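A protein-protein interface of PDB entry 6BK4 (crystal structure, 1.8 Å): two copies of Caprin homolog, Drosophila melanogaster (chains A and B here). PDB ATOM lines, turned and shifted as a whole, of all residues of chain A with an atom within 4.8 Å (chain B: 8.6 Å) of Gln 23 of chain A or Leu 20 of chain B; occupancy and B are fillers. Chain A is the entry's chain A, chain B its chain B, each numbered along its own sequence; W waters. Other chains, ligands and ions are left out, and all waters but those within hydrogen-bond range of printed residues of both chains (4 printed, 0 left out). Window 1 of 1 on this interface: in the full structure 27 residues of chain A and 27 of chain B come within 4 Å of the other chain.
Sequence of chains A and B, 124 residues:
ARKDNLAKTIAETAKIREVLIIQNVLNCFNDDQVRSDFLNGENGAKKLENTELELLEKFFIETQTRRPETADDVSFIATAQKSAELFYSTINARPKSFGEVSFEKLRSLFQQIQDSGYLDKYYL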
ATOM      1  N   VAL A  19       3.759  33.196   7.640  1.00  0.00           N
ATOM      2  CA  VAL A  19       2.860  32.078   7.926  1.00  0.00           C
ATOM      3  C   VAL A  19       3.633  30.765   7.901  1.00  0.00           C
ATOM      4  O   VAL A  19       3.501  29.923   8.801  1.00  0.00           O
ATOM      5  CB  VAL A  19       1.686  32.058   6.923  1.00  0.00           C
ATOM      6  CG1 VAL A  19       0.843  30.783   7.094  1.00  0.00           C
ATOM      7  CG2 VAL A  19       0.794  33.307   7.113  1.00  0.00           C
ATOM      8  N   LEU A  20       4.464  30.577   6.871  1.00  0.00           N
ATOM      9  CA  LEU A  20       5.218  29.319   6.759  1.00  0.00           C
ATOM     10  C   LEU A  20       6.203  29.153   7.908  1.00  0.00           C
ATOM     11  O   LEU A  20       6.419  28.032   8.402  1.00  0.00           O
ATOM     12  CB  LEU A  20       5.966  29.270   5.427  1.00  0.00           C
ATOM     13  CG  LEU A  20       5.067  29.243   4.187  1.00  0.00           C
ATOM     14  CD1 LEU A  20       5.949  29.380   2.915  1.00  0.00           C
ATOM     15  CD2 LEU A  20       4.233  27.979   4.149  1.00  0.00           C
ATOM     16  N   ILE A  21       6.836  30.247   8.327  1.00  0.00           N
ATOM     17  CA  ILE A  21       7.783  30.172   9.437  1.00  0.00           C
ATOM     18  C   ILE A  21       7.063  29.802  10.730  1.00  0.00           C
ATOM     19  O   ILE A  21       7.524  28.938  11.488  1.00  0.00           O
ATOM     20  CB  ILE A  21       8.556  31.499   9.569  1.00  0.00           C
ATOM     21  CG1 ILE A  21       9.518  31.658   8.379  1.00  0.00           C
ATOM     22  CG2 ILE A  21       9.309  31.568  10.931  1.00  0.00           C
ATOM     23  CD1 ILE A  21      10.108  33.056   8.266  1.00  0.00           C
ATOM     24  N   ILE A  22       5.926  30.458  11.002  1.00  0.00           N
ATOM     25  CA  ILE A  22       5.118  30.120  12.180  1.00  0.00           C
ATOM     26  C   ILE A  22       4.723  28.650  12.148  1.00  0.00           C
ATOM     27  O   ILE A  22       4.837  27.936  13.151  1.00  0.00           O
ATOM     28  CB  ILE A  22       3.876  31.029  12.258  1.00  0.00           C
ATOM     29  CG1 ILE A  22       4.295  32.480  12.534  1.00  0.00           C
ATOM     30  CG2 ILE A  22       2.850  30.479  13.265  1.00  0.00           C
ATOM     31  CD1 ILE A  22       3.163  33.499  12.334  1.00  0.00           C
ATOM     32  N   GLN A  23       4.247  28.171  10.992  1.00  0.00           N
ATOM     33  CA  GLN A  23       3.875  26.763  10.884  1.00  0.00           C
ATOM     34  C   GLN A  23       5.041  25.849  11.226  1.00  0.00           C
ATOM     35  O   GLN A  23       4.865  24.834  11.916  1.00  0.00           O
ATOM     36  CB  GLN A  23       3.366  26.453   9.476  1.00  0.00           C
ATOM     37  CG  GLN A  23       1.989  27.033   9.227  1.00  0.00           C
ATOM     38  CD  GLN A  23       1.542  26.812   7.803  1.00  0.00           C
ATOM     39  OE1 GLN A  23       2.372  26.723   6.899  1.00  0.00           O
ATOM     40  NE2 GLN A  23       0.235  26.720   7.596  1.00  0.00           N
ATOM     41  N   ASN A  24       6.237  26.182  10.735  1.00  0.00           N
ATOM     42  CA  ASN A  24       7.396  25.347  11.012  1.00  0.00           C
ATOM     43  C   ASN A  24       7.772  25.411  12.489  1.00  0.00           C
ATOM     44  O   ASN A  24       8.059  24.377  13.107  1.00  0.00           O
ATOM     45  CB  ASN A  24       8.570  25.775  10.139  1.00  0.00           C
ATOM     46  CG  ASN A  24       9.832  24.984  10.444  1.00  0.00           C
ATOM     47  OD1 ASN A  24      10.565  25.311  11.367  1.00  0.00           O
ATOM     48  ND2 ASN A  24      10.075  23.924   9.671  1.00  0.00           N
ATOM     49  N   VAL A  25       7.772  26.613  13.072  1.00  0.00           N
ATOM     50  CA  VAL A  25       8.064  26.738  14.501  1.00  0.00           C
ATOM     51  C   VAL A  25       7.122  25.858  15.306  1.00  0.00           C
ATOM     52  O   VAL A  25       7.551  25.108  16.195  1.00  0.00           O
ATOM     53  CB  VAL A  25       7.973  28.205  14.948  1.00  0.00           C
ATOM     54  CG1 VAL A  25       8.005  28.291  16.501  1.00  0.00           C
ATOM     55  CG2 VAL A  25       9.139  28.973  14.372  1.00  0.00           C
ATOM     56  N   LEU A  26       5.822  25.929  14.998  1.00  0.00           N
ATOM     57  CA  LEU A  26       4.854  25.127  15.739  1.00  0.00           C
ATOM     58  C   LEU A  26       5.128  23.643  15.554  1.00  0.00           C
ATOM     59  O   LEU A  26       5.002  22.859  16.503  1.00  0.00           O
ATOM     60  CB  LEU A  26       3.425  25.458  15.300  1.00  0.00           C
ATOM     61  CG  LEU A  26       2.901  26.853  15.641  1.00  0.00           C
ATOM     62  CD1 LEU A  26       1.605  27.122  14.864  1.00  0.00           C
ATOM     63  CD2 LEU A  26       2.666  26.995  17.143  1.00  0.00           C
ATOM     64  N   ASN A  27       5.508  23.237  14.340  1.00  0.00           N
ATOM     65  CA  ASN A  27       5.774  21.821  14.111  1.00  0.00           C
ATOM     66  C   ASN A  27       6.992  21.358  14.897  1.00  0.00           C
ATOM     67  O   ASN A  27       7.002  20.242  15.436  1.00  0.00           O
ATOM     68  CB  ASN A  27       5.936  21.550  12.617  1.00  0.00           C
ATOM     69  CG  ASN A  27       4.595  21.379  11.913  1.00  0.00           C
ATOM     70  OD1 ASN A  27       3.700  20.694  12.415  1.00  0.00           O
ATOM     71  ND2 ASN A  27       4.450  22.008  10.754  1.00  0.00           N
ATOM     72  N   THR A  65      -6.103  22.594   9.784  1.00  0.00           N
ATOM     73  CA  THR A  65      -7.273  22.474   8.947  1.00  0.00           C
ATOM     74  C   THR A  65      -7.648  21.002   8.999  1.00  0.00           C
ATOM     75  O   THR A  65      -6.827  20.175   9.271  1.00  0.00           O
ATOM     76  CB  THR A  65      -7.078  22.975   7.526  1.00  0.00           C
ATOM     77  OG1 THR A  65      -6.113  22.182   6.863  1.00  0.00           O
ATOM     78  CG2 THR A  65      -6.675  24.372   7.542  1.00  0.00           C
ATOM     79  N   ALA A  80     -10.450  26.083   7.605  1.00  0.00           N
ATOM     80  CA  ALA A  80      -9.486  26.888   6.854  1.00  0.00           C
ATOM     81  C   ALA A  80      -9.719  28.374   7.083  1.00  0.00           C
ATOM     82  O   ALA A  80      -8.763  29.146   7.230  1.00  0.00           O
ATOM     83  CB  ALA A  80      -9.567  26.570   5.361  1.00  0.00           C
ATOM     84  N   SER A  83      -8.509  29.232  10.621  1.00  0.00           N
ATOM     85  CA  SER A  83      -7.052  29.289  10.644  1.00  0.00           C
ATOM     86  C   SER A  83      -6.542  30.539   9.933  1.00  0.00           C
ATOM     87  O   SER A  83      -5.650  31.228  10.439  1.00  0.00           O
ATOM     88  CB  SER A  83      -6.473  28.020  10.015  1.00  0.00           C
ATOM     89  OG  SER A  83      -5.050  28.051  10.037  1.00  0.00           O
ATOM     90  N   ALA A  84      -7.111  30.861   8.759  1.00  0.00           N
ATOM     91  CA  ALA A  84      -6.669  32.048   8.023  1.00  0.00           C
ATOM     92  C   ALA A  84      -6.863  33.320   8.843  1.00  0.00           C
ATOM     93  O   ALA A  84      -5.993  34.199   8.854  1.00  0.00           O
ATOM     94  CB  ALA A  84      -7.410  32.165   6.693  1.00  0.00           C
ATOM     95  N   PHE A  87      -4.083  33.446  11.491  1.00  0.00           N
ATOM     96  CA  PHE A  87      -2.814  33.891  10.924  1.00  0.00           C
ATOM     97  C   PHE A  87      -2.864  35.371  10.555  1.00  0.00           C
ATOM     98  O   PHE A  87      -1.895  36.102  10.784  1.00  0.00           O
ATOM     99  CB  PHE A  87      -2.435  33.050   9.701  1.00  0.00           C
ATOM    100  CG  PHE A  87      -1.798  31.725  10.046  1.00  0.00           C
ATOM    101  CD1 PHE A  87      -0.554  31.677  10.671  1.00  0.00           C
ATOM    102  CD2 PHE A  87      -2.449  30.529   9.755  1.00  0.00           C
ATOM    103  CE1 PHE A  87       0.025  30.459  10.999  1.00  0.00           C
ATOM    104  CE2 PHE A  87      -1.872  29.311  10.059  1.00  0.00           C
ATOM    105  CZ  PHE A  87      -0.624  29.273  10.678  1.00  0.00           C
ATOM    106  N   THR B  13      -6.776  37.907   3.971  1.00  0.00           N
ATOM    107  CA  THR B  13      -7.188  36.672   4.628  1.00  0.00           C
ATOM    108  C   THR B  13      -7.523  35.592   3.604  1.00  0.00           C
ATOM    109  O   THR B  13      -7.179  34.415   3.792  1.00  0.00           O
ATOM    110  CB  THR B  13      -8.358  36.962   5.571  1.00  0.00           C
ATOM    111  OG1 THR B  13      -7.917  37.901   6.567  1.00  0.00           O
ATOM    112  CG2 THR B  13      -8.824  35.689   6.280  1.00  0.00           C
ATOM    113  N   ALA B  14      -8.150  35.983   2.487  1.00  0.00           N
ATOM    114  CA  ALA B  14      -8.450  35.023   1.426  1.00  0.00           C
ATOM    115  C   ALA B  14      -7.181  34.432   0.817  1.00  0.00           C
ATOM    116  O   ALA B  14      -7.168  33.257   0.426  1.00  0.00           O
ATOM    117  CB  ALA B  14      -9.308  35.685   0.340  1.00  0.00           C
ATOM    118  N   LYS B  15      -6.117  35.236   0.681  1.00  0.00           N
ATOM    119  CA  LYS B  15      -4.867  34.691   0.150  1.00  0.00           C
ATOM    120  C   LYS B  15      -4.269  33.673   1.111  1.00  0.00           C
ATOM    121  O   LYS B  15      -3.843  32.594   0.690  1.00  0.00           O
ATOM    122  CB  LYS B  15      -3.857  35.805  -0.134  1.00  0.00           C
ATOM    123  CG  LYS B  15      -4.198  36.647  -1.378  1.00  0.00           C
ATOM    124  CD  LYS B  15      -3.530  38.001  -1.315  1.00  0.00           C
ATOM    125  CE  LYS B  15      -3.764  38.790  -2.608  1.00  0.00           C
ATOM    126  NZ  LYS B  15      -3.186  38.071  -3.772  1.00  0.00           N
ATOM    127  N   ILE B  16      -4.251  33.992   2.413  1.00  0.00           N
ATOM    128  CA  ILE B  16      -3.783  33.027   3.408  1.00  0.00           C
ATOM    129  C   ILE B  16      -4.612  31.753   3.352  1.00  0.00           C
ATOM    130  O   ILE B  16      -4.080  30.638   3.416  1.00  0.00           O
ATOM    131  CB  ILE B  16      -3.815  33.654   4.814  1.00  0.00           C
ATOM    132  CG1 ILE B  16      -2.893  34.858   4.862  1.00  0.00           C
ATOM    133  CG2 ILE B  16      -3.382  32.630   5.863  1.00  0.00           C
ATOM    134  CD1 ILE B  16      -3.027  35.634   6.174  1.00  0.00           C
ATOM    135  N   ARG B  17      -5.924  31.888   3.209  1.00  0.00           N
ATOM    136  CA  ARG B  17      -6.764  30.700   3.196  1.00  0.00           C
ATOM    137  C   ARG B  17      -6.473  29.823   1.984  1.00  0.00           C
ATOM    138  O   ARG B  17      -6.499  28.593   2.086  1.00  0.00           O
ATOM    139  CB  ARG B  17      -8.240  31.094   3.226  1.00  0.00           C
ATOM    140  CG  ARG B  17      -9.121  29.925   3.576  1.00  0.00           C
ATOM    141  CD  ARG B  17     -10.583  30.324   3.585  1.00  0.00           C
ATOM    142  NE  ARG B  17     -11.139  30.340   2.239  1.00  0.00           N
ATOM    143  CZ  ARG B  17     -12.440  30.405   1.986  1.00  0.00           C
ATOM    144  NH1 ARG B  17     -13.306  30.476   2.989  1.00  0.00           N
ATOM    145  NH2 ARG B  17     -12.876  30.408   0.737  1.00  0.00           N
ATOM    146  N   GLU B  18      -6.201  30.427   0.828  1.00  0.00           N
ATOM    147  CA  GLU B  18      -5.915  29.604  -0.341  1.00  0.00           C
ATOM    148  C   GLU B  18      -4.638  28.801  -0.132  1.00  0.00           C
ATOM    149  O   GLU B  18      -4.576  27.622  -0.491  1.00  0.00           O
ATOM    150  CB  GLU B  18      -5.816  30.446  -1.612  1.00  0.00           C
ATOM    151  CG  GLU B  18      -5.730  29.534  -2.857  1.00  0.00           C
ATOM    152  CD  GLU B  18      -5.923  30.256  -4.178  1.00  0.00           C
ATOM    153  OE1 GLU B  18      -6.225  31.473  -4.166  1.00  0.00           O
ATOM    154  OE2 GLU B  18      -5.773  29.587  -5.228  1.00  0.00           O
ATOM    155  N   VAL B  19      -3.618  29.422   0.476  1.00  0.00           N
ATOM    156  CA  VAL B  19      -2.398  28.697   0.824  1.00  0.00           C
ATOM    157  C   VAL B  19      -2.727  27.519   1.731  1.00  0.00           C
ATOM    158  O   VAL B  19      -2.235  26.409   1.525  1.00  0.00           O
ATOM    159  CB  VAL B  19      -1.380  29.650   1.482  1.00  0.00           C
ATOM    160  CG1 VAL B  19      -0.228  28.853   2.094  1.00  0.00           C
ATOM    161  CG2 VAL B  19      -0.850  30.665   0.449  1.00  0.00           C
ATOM    162  N   LEU B  20      -3.558  27.747   2.761  1.00  0.00           N
ATOM    163  CA  LEU B  20      -3.891  26.662   3.687  1.00  0.00           C
ATOM    164  C   LEU B  20      -4.624  25.528   2.985  1.00  0.00           C
ATOM    165  O   LEU B  20      -4.401  24.353   3.290  1.00  0.00           O
ATOM    166  CB  LEU B  20      -4.747  27.179   4.857  1.00  0.00           C
ATOM    167  CG  LEU B  20      -4.056  28.187   5.768  1.00  0.00           C
ATOM    168  CD1 LEU B  20      -5.052  28.775   6.786  1.00  0.00           C
ATOM    169  CD2 LEU B  20      -2.866  27.521   6.511  1.00  0.00           C
ATOM    170  N   ILE B  21      -5.526  25.860   2.060  1.00  0.00           N
ATOM    171  CA  ILE B  21      -6.265  24.821   1.348  1.00  0.00           C
ATOM    172  C   ILE B  21      -5.329  24.005   0.464  1.00  0.00           C
ATOM    173  O   ILE B  21      -5.417  22.772   0.421  1.00  0.00           O
ATOM    174  CB  ILE B  21      -7.418  25.451   0.546  1.00  0.00           C
ATOM    175  CG1 ILE B  21      -8.434  26.050   1.522  1.00  0.00           C
ATOM    176  CG2 ILE B  21      -8.068  24.422  -0.378  1.00  0.00           C
ATOM    177  CD1 ILE B  21      -9.534  26.822   0.837  1.00  0.00           C
ATOM    178  N   ILE B  22      -4.417  24.672  -0.247  1.00  0.00           N
ATOM    179  CA  ILE B  22      -3.433  23.961  -1.064  1.00  0.00           C
ATOM    180  C   ILE B  22      -2.612  23.014  -0.194  1.00  0.00           C
ATOM    181  O   ILE B  22      -2.407  21.840  -0.539  1.00  0.00           O
ATOM    182  CB  ILE B  22      -2.543  24.970  -1.821  1.00  0.00           C
ATOM    183  CG1 ILE B  22      -3.366  25.716  -2.881  1.00  0.00           C
ATOM    184  CG2 ILE B  22      -1.313  24.298  -2.420  1.00  0.00           C
ATOM    185  CD1 ILE B  22      -2.650  26.898  -3.510  1.00  0.00           C
ATOM    186  N   GLN B  23      -2.142  23.501   0.959  1.00  0.00           N
ATOM    187  CA  GLN B  23      -1.346  22.646   1.839  1.00  0.00           C
ATOM    188  C   GLN B  23      -2.130  21.417   2.264  1.00  0.00           C
ATOM    189  O   GLN B  23      -1.583  20.311   2.314  1.00  0.00           O
ATOM    190  CB  GLN B  23      -0.889  23.423   3.068  1.00  0.00           C
ATOM    191  CG  GLN B  23       0.170  24.474   2.769  1.00  0.00           C
ATOM    192  CD  GLN B  23       0.479  25.291   4.004  1.00  0.00           C
ATOM    193  OE1 GLN B  23      -0.395  25.491   4.845  1.00  0.00           O
ATOM    194  NE2 GLN B  23       1.729  25.748   4.138  1.00  0.00           N
ATOM    195  N   ASN B  24      -3.415  21.592   2.568  1.00  0.00           N
ATOM    196  CA  ASN B  24      -4.228  20.448   2.952  1.00  0.00           C
ATOM    197  C   ASN B  24      -4.347  19.445   1.810  1.00  0.00           C
ATOM    198  O   ASN B  24      -4.193  18.236   2.016  1.00  0.00           O
ATOM    199  CB  ASN B  24      -5.605  20.910   3.397  1.00  0.00           C
ATOM    200  CG  ASN B  24      -6.500  19.750   3.752  1.00  0.00           C
ATOM    201  OD1 ASN B  24      -7.161  19.180   2.888  1.00  0.00           O
ATOM    202  ND2 ASN B  24      -6.509  19.378   5.030  1.00  0.00           N
ATOM    203  N   VAL B  25      -4.646  19.928   0.596  1.00  0.00           N
ATOM    204  CA  VAL B  25      -4.771  19.032  -0.554  1.00  0.00           C
ATOM    205  C   VAL B  25      -3.502  18.215  -0.721  1.00  0.00           C
ATOM    206  O   VAL B  25      -3.543  16.988  -0.897  1.00  0.00           O
ATOM    207  CB  VAL B  25      -5.082  19.831  -1.834  1.00  0.00           C
ATOM    208  CG1 VAL B  25      -4.953  18.934  -3.064  1.00  0.00           C
ATOM    209  CG2 VAL B  25      -6.485  20.446  -1.753  1.00  0.00           C
ATOM    210  N   LEU B  26      -2.351  18.893  -0.690  1.00  0.00           N
ATOM    211  CA  LEU B  26      -1.068  18.204  -0.795  1.00  0.00           C
ATOM    212  C   LEU B  26      -0.897  17.167   0.303  1.00  0.00           C
ATOM    213  O   LEU B  26      -0.426  16.052   0.045  1.00  0.00           O
ATOM    214  CB  LEU B  26       0.070  19.221  -0.737  1.00  0.00           C
ATOM    215  CG  LEU B  26       0.211  20.101  -1.972  1.00  0.00           C
ATOM    216  CD1 LEU B  26       1.169  21.252  -1.704  1.00  0.00           C
ATOM    217  CD2 LEU B  26       0.687  19.279  -3.151  1.00  0.00           C
ATOM    218  N   ASN B  27      -1.259  17.516   1.539  1.00  0.00           N
ATOM    219  CA  ASN B  27      -1.064  16.573   2.637  1.00  0.00           C
ATOM    220  C   ASN B  27      -1.969  15.355   2.495  1.00  0.00           C
ATOM    221  O   ASN B  27      -1.576  14.249   2.877  1.00  0.00           O
ATOM    222  CB  ASN B  27      -1.293  17.267   3.977  1.00  0.00           C
ATOM    223  CG  ASN B  27      -0.193  18.275   4.307  1.00  0.00           C
ATOM    224  OD1 ASN B  27       0.957  18.116   3.889  1.00  0.00           O
ATOM    225  ND2 ASN B  27      -0.543  19.310   5.068  1.00  0.00           N
ATOM    226  N   THR B  63       7.605  23.328  -1.859  1.00  0.00           N
ATOM    227  CA  THR B  63       6.954  24.168  -0.855  1.00  0.00           C
ATOM    228  C   THR B  63       7.219  23.701   0.566  1.00  0.00           C
ATOM    229  O   THR B  63       6.739  24.342   1.512  1.00  0.00           O
ATOM    230  CB  THR B  63       5.425  24.262  -1.082  1.00  0.00           C
ATOM    231  OG1 THR B  63       4.841  22.959  -1.143  1.00  0.00           O
ATOM    232  CG2 THR B  63       5.090  25.047  -2.363  1.00  0.00           C
ATOM    233  N   THR B  65       9.288  23.482   3.873  1.00  0.00           N
ATOM    234  CA  THR B  65      10.336  24.243   4.498  1.00  0.00           C
ATOM    235  C   THR B  65      11.070  23.220   5.353  1.00  0.00           C
ATOM    236  O   THR B  65      10.488  22.278   5.776  1.00  0.00           O
ATOM    237  CB  THR B  65       9.816  25.400   5.344  1.00  0.00           C
ATOM    238  OG1 THR B  65       9.127  24.886   6.457  1.00  0.00           O
ATOM    239  CG2 THR B  65       8.898  26.228   4.551  1.00  0.00           C
ATOM    240  N   ARG B  67      14.439  22.673   8.335  1.00  0.00           N
ATOM    241  CA  ARG B  67      15.575  23.091   9.128  1.00  0.00           C
ATOM    242  C   ARG B  67      16.694  22.191   8.653  1.00  0.00           C
ATOM    243  O   ARG B  67      16.522  21.016   8.510  1.00  0.00           O
ATOM    244  CB  ARG B  67      15.348  22.900  10.606  1.00  0.00           C
ATOM    245  CG  ARG B  67      14.190  23.665  11.200  1.00  0.00           C
ATOM    246  CD  ARG B  67      14.466  25.142  11.387  1.00  0.00           C
ATOM    247  NE  ARG B  67      13.261  25.863  11.709  1.00  0.00           N
ATOM    248  CZ  ARG B  67      13.207  27.128  12.058  1.00  0.00           C
ATOM    249  NH1 ARG B  67      14.300  27.828  12.141  1.00  0.00           N
ATOM    250  NH2 ARG B  67      12.060  27.692  12.312  1.00  0.00           N
ATOM    251  N   PHE B  76      17.254  27.269   6.294  1.00  0.00           N
ATOM    252  CA  PHE B  76      15.811  27.200   6.556  1.00  0.00           C
ATOM    253  C   PHE B  76      15.117  28.362   5.862  1.00  0.00           C
ATOM    254  O   PHE B  76      14.112  28.182   5.181  1.00  0.00           O
ATOM    255  CB  PHE B  76      15.500  27.251   8.039  1.00  0.00           C
ATOM    256  CG  PHE B  76      14.055  27.483   8.318  1.00  0.00           C
ATOM    257  CD1 PHE B  76      13.133  26.464   8.124  1.00  0.00           C
ATOM    258  CD2 PHE B  76      13.603  28.724   8.753  1.00  0.00           C
ATOM    259  CE1 PHE B  76      11.782  26.671   8.367  1.00  0.00           C
ATOM    260  CE2 PHE B  76      12.239  28.934   8.996  1.00  0.00           C
ATOM    261  CZ  PHE B  76      11.340  27.914   8.798  1.00  0.00           C
ATOM    262  N   SER B  83       9.491  28.560  -0.866  1.00  0.00           N
ATOM    263  CA  SER B  83       8.109  28.109  -0.745  1.00  0.00           C
ATOM    264  C   SER B  83       7.135  29.282  -0.865  1.00  0.00           C
ATOM    265  O   SER B  83       6.126  29.200  -1.571  1.00  0.00           O
ATOM    266  CB  SER B  83       7.925  27.379   0.587  1.00  0.00           C
ATOM    267  OG  SER B  83       6.574  26.986   0.756  1.00  0.00           O
ATOM    268  N   PHE B  87       4.106  29.801  -3.583  1.00  0.00           N
ATOM    269  CA  PHE B  87       2.719  30.054  -3.207  1.00  0.00           C
ATOM    270  C   PHE B  87       2.236  31.373  -3.784  1.00  0.00           C
ATOM    271  O   PHE B  87       1.117  31.454  -4.296  1.00  0.00           O
ATOM    272  CB  PHE B  87       2.544  30.052  -1.677  1.00  0.00           C
ATOM    273  CG  PHE B  87       2.377  28.681  -1.079  1.00  0.00           C
ATOM    274  CD1 PHE B  87       1.279  27.904  -1.389  1.00  0.00           C
ATOM    275  CD2 PHE B  87       3.309  28.191  -0.172  1.00  0.00           C
ATOM    276  CE1 PHE B  87       1.114  26.635  -0.821  1.00  0.00           C
ATOM    277  CE2 PHE B  87       3.164  26.949   0.387  1.00  0.00           C
ATOM    278  CZ  PHE B  87       2.066  26.161   0.072  1.00  0.00           C
ATOM    279  N   ILE B  91      -1.049  31.516  -6.198  1.00  0.00           N
ATOM    280  CA  ILE B  91      -2.335  32.112  -5.857  1.00  0.00           C
ATOM    281  C   ILE B  91      -2.594  33.410  -6.608  1.00  0.00           C
ATOM    282  O   ILE B  91      -3.727  33.885  -6.613  1.00  0.00           O
ATOM    283  CB  ILE B  91      -2.473  32.336  -4.335  1.00  0.00           C
ATOM    284  CG1 ILE B  91      -1.501  33.396  -3.831  1.00  0.00           C
ATOM    285  CG2 ILE B  91      -2.239  31.029  -3.602  1.00  0.00           C
ATOM    286  CD1 ILE B  91      -1.686  33.718  -2.309  1.00  0.00           C
ATOM    287  N   GLN B 114     -10.315  20.855  -5.167  1.00  0.00           N
ATOM    288  CA  GLN B 114     -11.152  21.342  -4.075  1.00  0.00           C
ATOM    289  C   GLN B 114     -12.619  21.402  -4.491  1.00  0.00           C
ATOM    290  O   GLN B 114     -13.504  21.015  -3.720  1.00  0.00           O
ATOM    291  CB  GLN B 114     -10.637  22.707  -3.605  1.00  0.00           C
ATOM    292  CG  GLN B 114     -11.487  23.372  -2.531  1.00  0.00           C
ATOM    293  CD  GLN B 114     -11.491  22.610  -1.216  1.00  0.00           C
ATOM    294  OE1 GLN B 114     -10.648  21.735  -0.973  1.00  0.00           O
ATOM    295  NE2 GLN B 114     -12.457  22.926  -0.372  1.00  0.00           N
HETATM  296  O   HOH W   1      -3.978  23.372   5.746  1.00  0.00           O
HETATM  297  O   HOH W   2      -1.593  23.939   6.871  1.00  0.00           O
HETATM  298  O   HOH W   3      11.850  21.420   9.802  1.00  0.00           O
HETATM  299  O   HOH W   4       6.367  25.601   7.043  1.00  0.00           O
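OE1 of Gln 23 of chain A lies within hydrogen-bond range of NE2 of Gln 23 of chain B (3.0 Å).
The side-chain amide nitrogen (ND2) of Asn 24 of chain A sits at hydrogen-bond distance from the side-chain hydroxyl (OG1) of Thr 65 of chain B (3.5 Å).
NE of Arg 67 of chain B is in hydrogen-bond range of OD1 of Asn 24 of chain A, at 2.8 Å.
OG1 of Thr 65 of chain A lies within hydrogen-bond range of ND2 of Asn 24 of chain B (3.4 Å).
The side-chain amide nitrogen (ND2) of Asn 27 of chain A lies within hydrogen-bond range of the backbone carbonyl oxygen (O) of Gln 23 of chain A (3.1 Å).
The backbone carbonyl oxygen of Gln 23 of chain B sits at hydrogen-bond distance from the side-chain amide nitrogen of Asn 27 of chain B.
The side-chain hydroxyl of Ser 83 of chain B sits at hydrogen-bond distance from the backbone carbonyl oxygen of Thr 63 of chain B, 2.8 Å away.
Among the printed residues, merely in contact across the chains: Leu 20 of chain A with Ser 83 of chain B (3.3 Å), Asn 24 of chain A with Phe 76 of chain B (3.3 Å), Ser 83 of chain A with Leu 20 of chain B (3.3 Å), Leu 20 of chain A with Gln 23 of chain B (3.4 Å), Gln 23 of chain A with Leu 20 of chain B (3.4 Å), Ala 84 of chain A with Leu 20 of chain B (3.5 Å), Ala 84 of chain A with Thr 13 of chain B (3.7 Å), Ala 84 of chain A with Arg 17 of chain B (3.7 Å), Ala 80 of chain A with Arg 17 of chain B (3.8 Å), Ala 80 of chain A with Leu 20 of chain B (3.8 Å), Val 25 of chain A with Arg 67 of chain B (3.8 Å), Ile 21 of chain A with Phe 76 of chain B (3.9 Å), Phe 87 of chain A with Ile 16 of chain B (3.98 Å) and Ala 84 of chain A with Ile 16 of chain B (3.98 Å).
Of chain B, only Leu 20 and Gln 23 come within 4 Å of Gln 23 of chain A.
Of the printed residues of chain A, Ile 16 of chain B touches Ala 84 (3.98 Å) and Phe 87 (3.98 Å).
Of the printed residues of chain B, Phe 87 of chain A touches Ile 16.
Of the printed residues of chain B, Val 25 of chain A touches Arg 67 (3.8 Å).
Of the printed residues of chain B, Ala 80 of chain A touches Arg 17 and Leu 20.
Ile 22 of chain B touches none of the printed residues of chain A.
Leu 26 of chain A touches none of the printed residues of chain B.
The nearest residue of chain A that does not touch Leu 20 of chain B is Phe 87 of chain A (4.1 Å).
Of the 23 printed residues of chain B, 10 touch a printed residue of chain A.
Of the 14 printed residues of chain A, 10 touch a printed residue of chain B.
Hydrophobic or aromatic side chains of chain A that line the printed part of chain B: Leu 20, Ile 21, Val 25, Ala 80, Ala 84 and Phe 87.
Among the printed residues, no Asp or Glu carboxylate lies within 4 Å of a Lys or Arg side-chain nitrogen of the other chain.
Leu 20 of chain A touches Gln 23 of chain B, and with the chains exchanged Gln 23 of chain A touches Leu 20 of chain B.
Leu 20 of chain A touches Ser 83 of chain B, and with the chains exchanged Ser 83 of chain A touches Leu 20 of chain B.
Gln 23 of chain B touches its own counterpart, Gln 23 of chain A.
Positions printed for both chains: 19, 20, 21, 22, 23, 24, 25, 26, 27, 65, 83 and 87.
Water W1 lies within hydrogen-bond range of the backbone carbonyl oxygen (O) of Leu 20 of chain B (2.7 Å) and the side-chain hydroxyl (OG1) of Thr 65 of chain A (2.7 Å).
Water W2 bridges the side-chain amide oxygen (OE1) of Gln 23 of chain B (2.8 Å) and the side-chain amide nitrogen (NE2) of Gln 23 of chain A (3.4 Å).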
